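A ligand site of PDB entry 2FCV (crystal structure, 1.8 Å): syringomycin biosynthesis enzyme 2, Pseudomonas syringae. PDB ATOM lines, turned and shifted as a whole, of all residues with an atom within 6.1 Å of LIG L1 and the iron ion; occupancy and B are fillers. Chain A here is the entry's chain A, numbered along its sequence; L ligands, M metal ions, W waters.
The backbone NH of Thr 116 sits at hydrogen-bond distance from the side-chain hydroxyl of Ser 240. The side-chain hydroxyl of Thr 116 sits at hydrogen-bond distance from the side-chain amino group of Lys 109. NH2 of Arg 257 sits at hydrogen-bond distance from OG1 of Thr 146. O of Phe 107 is in hydrogen-bond range of NH2 of Arg 251, 2.9 Å away. The backbone carbonyl oxygen (O) of Arg 251 sits at hydrogen-bond distance from the backbone NH (N) of Lys 109, 2.9 Å away. O of Gly 159 sits at hydrogen-bond distance from NH1 of Arg 251, at 2.6 Å. The backbone carbonyl oxygen of Gly 253 is in hydrogen-bond range of the backbone NH of Phe 107 (2.8 Å). N of Thr 146 lies within hydrogen-bond range of O of Phe 232 (2.8 Å).
The iron ion is bound by an oxygen (O2) of LIG L1 (2.0 Å), a ring nitrogen (NE2) of His 119 (2.1 Å), an oxygen (O3) of LIG L1 (2.2 Å), a ring nitrogen (NE2) of His 238 (2.3 Å), water W2 (2.3 Å) and a bromine (BR1) of LG2 L2 (2.5 Å).
Phe 107 touches LIG L1. Lys 109 touches LIG L1. Thr 146 touches LIG L1. CD2 of Leu 161 touches O5 of LIG L1, 3.6 Å away. Phe 232 touches LIG L1. Ser 240 touches LIG L1. CB of Ala 255 touches O1 of LIG L1, 3.7 Å away. Hydrophobic or aromatic side chains that line LIG L1: Phe 107, His 119, Trp 148, Leu 161, Phe 232, His 238 and Ala 255. Of the 22 residues printed, 13 come within 4 Å of LIG L1. Along chain A the residues within 4 Å of LIG L1 span positions 107 to 257. The nearest printed residue that does not touch LIG L1 is Phe 199 (4.7 Å).
OG1 of Thr 116 sits at hydrogen-bond distance from O4 of LIG L1 (2.6 Å). NH2 of Arg 257 is in salt-bridge range of O1 of LIG L1, at 3.7 Å. The guanidinium group of Arg 251 is in salt-bridge range of an oxygen (O5) of LIG L1 (2.9 Å). The indole nitrogen of Trp 148 is in hydrogen-bond range of an oxygen (O5) of LIG L1 (2.9 Å).
Along chain A the residues within 4 Å of the iron ion span positions 119 to 238. The nearest printed residue that does not touch the iron ion is Arg 257 (4.2 Å).
Water W1 bridges the side-chain hydroxyl of Thr 146 (2.8 Å) and the guanidinium group of Arg 257 (3.0 Å).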
ATOM      1  N   PHE A 107      14.210  -4.848   0.425  1.00  0.00           N
ATOM      2  CA  PHE A 107      14.197  -4.731   1.878  1.00  0.00           C
ATOM      3  C   PHE A 107      15.324  -5.620   2.395  1.00  0.00           C
ATOM      4  O   PHE A 107      15.129  -6.775   2.702  1.00  0.00           O
ATOM      5  CB  PHE A 107      12.878  -5.196   2.515  1.00  0.00           C
ATOM      6  CG  PHE A 107      11.733  -4.192   2.360  1.00  0.00           C
ATOM      7  CD1 PHE A 107      10.805  -4.330   1.340  1.00  0.00           C
ATOM      8  CD2 PHE A 107      11.593  -3.154   3.251  1.00  0.00           C
ATOM      9  CE1 PHE A 107       9.753  -3.404   1.170  1.00  0.00           C
ATOM     10  CE2 PHE A 107      10.524  -2.203   3.121  1.00  0.00           C
ATOM     11  CZ  PHE A 107       9.604  -2.345   2.065  1.00  0.00           C
ATOM     12  N   PRO A 108      16.524  -5.042   2.493  1.00  0.00           N
ATOM     13  CA  PRO A 108      17.616  -5.705   3.180  1.00  0.00           C
ATOM     14  C   PRO A 108      17.514  -5.628   4.717  1.00  0.00           C
ATOM     15  O   PRO A 108      17.107  -4.603   5.299  1.00  0.00           O
ATOM     16  CB  PRO A 108      18.824  -4.962   2.656  1.00  0.00           C
ATOM     17  CG  PRO A 108      18.321  -3.519   2.467  1.00  0.00           C
ATOM     18  CD  PRO A 108      16.909  -3.733   1.933  1.00  0.00           C
ATOM     19  N   LYS A 109      17.890  -6.705   5.372  1.00  0.00           N
ATOM     20  CA  LYS A 109      18.281  -6.655   6.771  1.00  0.00           C
ATOM     21  C   LYS A 109      19.690  -7.181   6.835  1.00  0.00           C
ATOM     22  O   LYS A 109      19.949  -8.373   6.662  1.00  0.00           O
ATOM     23  CB  LYS A 109      17.394  -7.464   7.693  1.00  0.00           C
ATOM     24  CG  LYS A 109      15.971  -6.983   7.812  1.00  0.00           C
ATOM     25  CD  LYS A 109      15.849  -5.671   8.553  1.00  0.00           C
ATOM     26  CE  LYS A 109      14.413  -5.164   8.492  1.00  0.00           C
ATOM     27  NZ  LYS A 109      14.313  -3.830   9.080  1.00  0.00           N
ATOM     28  N   GLY A 115      14.439  -4.340  13.619  1.00  0.00           N
ATOM     29  CA  GLY A 115      13.239  -4.809  12.982  1.00  0.00           C
ATOM     30  C   GLY A 115      12.489  -3.666  12.323  1.00  0.00           C
ATOM     31  O   GLY A 115      12.574  -2.517  12.741  1.00  0.00           O
ATOM     32  N   THR A 116      11.701  -3.981  11.336  1.00  0.00           N
ATOM     33  CA  THR A 116      10.814  -2.999  10.711  1.00  0.00           C
ATOM     34  C   THR A 116       9.680  -2.675  11.682  1.00  0.00           C
ATOM     35  O   THR A 116       9.113  -3.571  12.282  1.00  0.00           O
ATOM     36  CB  THR A 116      10.276  -3.514   9.406  1.00  0.00           C
ATOM     37  OG1 THR A 116      11.376  -3.680   8.475  1.00  0.00           O
ATOM     38  CG2 THR A 116       9.360  -2.493   8.802  1.00  0.00           C
ATOM     39  N   HIS A 119       3.399  -1.233  10.995  1.00  0.00           N
ATOM     40  CA  HIS A 119       2.801  -0.251  10.101  1.00  0.00           C
ATOM     41  C   HIS A 119       1.679  -0.843   9.272  1.00  0.00           C
ATOM     42  O   HIS A 119       1.548  -2.044   9.138  1.00  0.00           O
ATOM     43  CB  HIS A 119       3.865   0.437   9.228  1.00  0.00           C
ATOM     44  CG  HIS A 119       4.512  -0.448   8.219  1.00  0.00           C
ATOM     45  ND1 HIS A 119       5.404  -1.464   8.560  1.00  0.00           N
ATOM     46  CD2 HIS A 119       4.437  -0.461   6.877  1.00  0.00           C
ATOM     47  CE1 HIS A 119       5.805  -2.072   7.461  1.00  0.00           C
ATOM     48  NE2 HIS A 119       5.271  -1.447   6.424  1.00  0.00           N
ATOM     49  N   PHE A 124      -0.105   5.496   0.837  1.00  0.00           N
ATOM     50  CA  PHE A 124       1.340   5.665   0.682  1.00  0.00           C
ATOM     51  C   PHE A 124       1.780   7.151   0.713  1.00  0.00           C
ATOM     52  O   PHE A 124       2.842   7.519   0.181  1.00  0.00           O
ATOM     53  CB  PHE A 124       1.853   4.887  -0.568  1.00  0.00           C
ATOM     54  CG  PHE A 124       1.970   3.422  -0.340  1.00  0.00           C
ATOM     55  CD1 PHE A 124       3.203   2.820  -0.175  1.00  0.00           C
ATOM     56  CD2 PHE A 124       0.817   2.630  -0.242  1.00  0.00           C
ATOM     57  CE1 PHE A 124       3.296   1.458   0.059  1.00  0.00           C
ATOM     58  CE2 PHE A 124       0.903   1.280   0.016  1.00  0.00           C
ATOM     59  CZ  PHE A 124       2.114   0.697   0.157  1.00  0.00           C
ATOM     60  N   THR A 146       0.725  -6.502  -1.638  1.00  0.00           N
ATOM     61  CA  THR A 146       2.178  -6.667  -1.630  1.00  0.00           C
ATOM     62  C   THR A 146       2.502  -8.143  -1.787  1.00  0.00           C
ATOM     63  O   THR A 146       1.972  -8.994  -1.052  1.00  0.00           O
ATOM     64  CB  THR A 146       2.776  -6.076  -0.354  1.00  0.00           C
ATOM     65  OG1 THR A 146       2.561  -4.670  -0.384  1.00  0.00           O
ATOM     66  CG2 THR A 146       4.270  -6.352  -0.262  1.00  0.00           C
ATOM     67  N   TRP A 148       5.786 -10.268  -1.317  1.00  0.00           N
ATOM     68  CA  TRP A 148       7.124 -10.125  -0.770  1.00  0.00           C
ATOM     69  C   TRP A 148       7.845 -11.438  -1.008  1.00  0.00           C
ATOM     70  O   TRP A 148       7.467 -12.480  -0.484  1.00  0.00           O
ATOM     71  CB  TRP A 148       7.016  -9.745   0.702  1.00  0.00           C
ATOM     72  CG  TRP A 148       8.254  -9.382   1.469  1.00  0.00           C
ATOM     73  CD1 TRP A 148       8.596  -8.154   1.880  1.00  0.00           C
ATOM     74  CD2 TRP A 148       9.221 -10.293   2.057  1.00  0.00           C
ATOM     75  NE1 TRP A 148       9.731  -8.211   2.666  1.00  0.00           N
ATOM     76  CE2 TRP A 148      10.135  -9.503   2.783  1.00  0.00           C
ATOM     77  CE3 TRP A 148       9.387 -11.671   2.042  1.00  0.00           C
ATOM     78  CZ2 TRP A 148      11.211 -10.056   3.517  1.00  0.00           C
ATOM     79  CZ3 TRP A 148      10.471 -12.228   2.739  1.00  0.00           C
ATOM     80  CH2 TRP A 148      11.360 -11.407   3.475  1.00  0.00           C
ATOM     81  N   GLY A 159      15.449 -11.718  10.723  1.00  0.00           N
ATOM     82  CA  GLY A 159      14.520 -10.654  10.461  1.00  0.00           C
ATOM     83  C   GLY A 159      13.337 -10.896   9.567  1.00  0.00           C
ATOM     84  O   GLY A 159      12.975 -10.020   8.772  1.00  0.00           O
ATOM     85  N   LEU A 161       9.400 -11.488   8.293  1.00  0.00           N
ATOM     86  CA  LEU A 161       8.196 -10.729   8.523  1.00  0.00           C
ATOM     87  C   LEU A 161       7.363 -11.307   9.663  1.00  0.00           C
ATOM     88  O   LEU A 161       7.432 -12.489   9.987  1.00  0.00           O
ATOM     89  CB  LEU A 161       7.344 -10.730   7.236  1.00  0.00           C
ATOM     90  CG  LEU A 161       7.983 -10.033   6.045  1.00  0.00           C
ATOM     91  CD1 LEU A 161       6.935  -9.972   4.905  1.00  0.00           C
ATOM     92  CD2 LEU A 161       8.471  -8.648   6.353  1.00  0.00           C
ATOM     93  N   PHE A 198      11.715   2.592  11.114  1.00  0.00           N
ATOM     94  CA  PHE A 198      11.123   2.621   9.788  1.00  0.00           C
ATOM     95  C   PHE A 198      12.038   3.350   8.825  1.00  0.00           C
ATOM     96  O   PHE A 198      11.670   4.382   8.277  1.00  0.00           O
ATOM     97  CB  PHE A 198       9.732   3.246   9.844  1.00  0.00           C
ATOM     98  CG  PHE A 198       8.880   2.933   8.656  1.00  0.00           C
ATOM     99  CD1 PHE A 198       8.331   1.676   8.510  1.00  0.00           C
ATOM    100  CD2 PHE A 198       8.637   3.884   7.685  1.00  0.00           C
ATOM    101  CE1 PHE A 198       7.534   1.369   7.418  1.00  0.00           C
ATOM    102  CE2 PHE A 198       7.845   3.571   6.581  1.00  0.00           C
ATOM    103  CZ  PHE A 198       7.293   2.299   6.459  1.00  0.00           C
ATOM    104  N   PHE A 199      13.233   2.812   8.611  1.00  0.00           N
ATOM    105  CA  PHE A 199      14.118   3.295   7.551  1.00  0.00           C
ATOM    106  C   PHE A 199      14.468   4.776   7.730  1.00  0.00           C
ATOM    107  O   PHE A 199      14.641   5.496   6.752  1.00  0.00           O
ATOM    108  CB  PHE A 199      13.487   3.011   6.168  1.00  0.00           C
ATOM    109  CG  PHE A 199      12.904   1.632   6.074  1.00  0.00           C
ATOM    110  CD1 PHE A 199      11.536   1.441   6.197  1.00  0.00           C
ATOM    111  CD2 PHE A 199      13.739   0.513   5.975  1.00  0.00           C
ATOM    112  CE1 PHE A 199      10.996   0.153   6.202  1.00  0.00           C
ATOM    113  CE2 PHE A 199      13.208  -0.774   5.965  1.00  0.00           C
ATOM    114  CZ  PHE A 199      11.828  -0.953   6.103  1.00  0.00           C
ATOM    115  N   PHE A 232       0.077 -10.233   0.817  1.00  0.00           N
ATOM    116  CA  PHE A 232      -0.684  -9.555   1.874  1.00  0.00           C
ATOM    117  C   PHE A 232      -1.119  -8.152   1.470  1.00  0.00           C
ATOM    118  O   PHE A 232      -0.496  -7.461   0.647  1.00  0.00           O
ATOM    119  CB  PHE A 232       0.068  -9.515   3.236  1.00  0.00           C
ATOM    120  CG  PHE A 232       1.404  -8.766   3.213  1.00  0.00           C
ATOM    121  CD1 PHE A 232       1.499  -7.497   3.720  1.00  0.00           C
ATOM    122  CD2 PHE A 232       2.539  -9.363   2.700  1.00  0.00           C
ATOM    123  CE1 PHE A 232       2.690  -6.809   3.719  1.00  0.00           C
ATOM    124  CE2 PHE A 232       3.758  -8.684   2.687  1.00  0.00           C
ATOM    125  CZ  PHE A 232       3.841  -7.417   3.199  1.00  0.00           C
ATOM    126  N   SER A 234      -1.332  -4.219   2.110  1.00  0.00           N
ATOM    127  CA  SER A 234      -0.503  -3.240   2.757  1.00  0.00           C
ATOM    128  C   SER A 234      -1.200  -2.650   3.974  1.00  0.00           C
ATOM    129  O   SER A 234      -0.563  -2.112   4.854  1.00  0.00           O
ATOM    130  CB  SER A 234      -0.078  -2.126   1.784  1.00  0.00           C
ATOM    131  OG  SER A 234      -1.189  -1.346   1.384  1.00  0.00           O
ATOM    132  N   HIS A 238       1.759  -5.169   9.710  1.00  0.00           N
ATOM    133  CA  HIS A 238       2.927  -5.984   9.464  1.00  0.00           C
ATOM    134  C   HIS A 238       4.193  -5.255   9.931  1.00  0.00           C
ATOM    135  O   HIS A 238       4.195  -4.033  10.065  1.00  0.00           O
ATOM    136  CB  HIS A 238       2.959  -6.411   7.962  1.00  0.00           C
ATOM    137  CG  HIS A 238       3.144  -5.274   7.005  1.00  0.00           C
ATOM    138  ND1 HIS A 238       2.162  -4.339   6.728  1.00  0.00           N
ATOM    139  CD2 HIS A 238       4.182  -4.972   6.180  1.00  0.00           C
ATOM    140  CE1 HIS A 238       2.607  -3.469   5.844  1.00  0.00           C
ATOM    141  NE2 HIS A 238       3.830  -3.840   5.479  1.00  0.00           N
ATOM    142  N   ALA A 239       5.264  -6.051  10.163  1.00  0.00           N
ATOM    143  CA  ALA A 239       6.516  -5.607  10.713  1.00  0.00           C
ATOM    144  C   ALA A 239       7.534  -6.682  10.391  1.00  0.00           C
ATOM    145  O   ALA A 239       7.248  -7.610   9.648  1.00  0.00           O
ATOM    146  CB  ALA A 239       6.438  -5.411  12.246  1.00  0.00           C
ATOM    147  N   SER A 240       8.740  -6.538  10.908  1.00  0.00           N
ATOM    148  CA  SER A 240       9.708  -7.636  10.838  1.00  0.00           C
ATOM    149  C   SER A 240      10.406  -7.769  12.165  1.00  0.00           C
ATOM    150  O   SER A 240      10.525  -6.784  12.946  1.00  0.00           O
ATOM    151  CB  SER A 240      10.756  -7.368   9.738  1.00  0.00           C
ATOM    152  OG  SER A 240      11.916  -6.686  10.230  1.00  0.00           O
ATOM    153  N   ARG A 251      19.557 -10.794   5.153  1.00  0.00           N
ATOM    154  CA  ARG A 251      18.251 -11.198   4.658  1.00  0.00           C
ATOM    155  C   ARG A 251      17.866 -10.223   3.552  1.00  0.00           C
ATOM    156  O   ARG A 251      18.081  -9.007   3.670  1.00  0.00           O
ATOM    157  CB  ARG A 251      17.196 -11.132   5.791  1.00  0.00           C
ATOM    158  CG  ARG A 251      15.786 -11.412   5.358  1.00  0.00           C
ATOM    159  CD  ARG A 251      15.060 -10.106   4.911  1.00  0.00           C
ATOM    160  NE  ARG A 251      14.304  -9.544   6.002  1.00  0.00           N
ATOM    161  CZ  ARG A 251      13.546  -8.464   5.938  1.00  0.00           C
ATOM    162  NH1 ARG A 251      12.868  -8.095   7.004  1.00  0.00           N
ATOM    163  NH2 ARG A 251      13.495  -7.741   4.828  1.00  0.00           N
ATOM    164  N   GLY A 253      14.471  -9.283   1.193  1.00  0.00           N
ATOM    165  CA  GLY A 253      13.150  -9.400   0.605  1.00  0.00           C
ATOM    166  C   GLY A 253      13.010  -8.454  -0.563  1.00  0.00           C
ATOM    167  O   GLY A 253      13.650  -7.385  -0.591  1.00  0.00           O
ATOM    168  N   ALA A 255       9.799  -6.752  -2.477  1.00  0.00           N
ATOM    169  CA  ALA A 255       8.367  -6.431  -2.533  1.00  0.00           C
ATOM    170  C   ALA A 255       7.955  -5.932  -3.913  1.00  0.00           C
ATOM    171  O   ALA A 255       8.563  -5.031  -4.455  1.00  0.00           O
ATOM    172  CB  ALA A 255       7.994  -5.358  -1.465  1.00  0.00           C
ATOM    173  N   ARG A 257       4.389  -4.468  -5.630  1.00  0.00           N
ATOM    174  CA  ARG A 257       3.134  -3.912  -5.172  1.00  0.00           C
ATOM    175  C   ARG A 257       2.195  -3.737  -6.353  1.00  0.00           C
ATOM    176  O   ARG A 257       2.583  -3.138  -7.354  1.00  0.00           O
ATOM    177  CB  ARG A 257       3.397  -2.585  -4.457  1.00  0.00           C
ATOM    178  CG  ARG A 257       4.379  -2.738  -3.241  1.00  0.00           C
ATOM    179  CD  ARG A 257       4.348  -1.466  -2.363  1.00  0.00           C
ATOM    180  NE  ARG A 257       5.485  -1.276  -1.415  1.00  0.00           N
ATOM    181  CZ  ARG A 257       5.551  -1.799  -0.189  1.00  0.00           C
ATOM    182  NH1 ARG A 257       6.571  -1.525   0.633  1.00  0.00           N
ATOM    183  NH2 ARG A 257       4.618  -2.629   0.230  1.00  0.00           N
HETATM  184  C1  LIG L   1       6.477  -4.325   2.918  1.00  0.00           C
HETATM  185  O1  LIG L   1       6.744  -5.148   1.995  1.00  0.00           O
HETATM  186  O2  LIG L   1       5.509  -3.538   2.826  1.00  0.00           O
HETATM  187  C2  LIG L   1       7.315  -4.288   4.134  1.00  0.00           C
HETATM  188  O3  LIG L   1       7.017  -3.520   5.018  1.00  0.00           O
HETATM  189  C3  LIG L   1       8.503  -5.235   4.322  1.00  0.00           C
HETATM  190  C4  LIG L   1       9.310  -4.911   5.605  1.00  0.00           C
HETATM  191  C5  LIG L   1      10.595  -5.701   5.668  1.00  0.00           C
HETATM  192  O4  LIG L   1      11.329  -5.567   6.674  1.00  0.00           O
HETATM  193  O5  LIG L   1      10.881  -6.469   4.724  1.00  0.00           O
HETATM  194 BR1  LG2 L   2       3.358  -0.986   3.461  1.00  0.00          BR
HETATM  195 FE    FE M   1       5.223  -2.369   4.485  1.00  0.00          FE
HETATM  196  O   HOH W   1       2.676  -3.753   2.289  1.00  0.00           O
HETATM  197  O   HOH W   2       6.534  -0.704   3.704  1.00  0.00           O
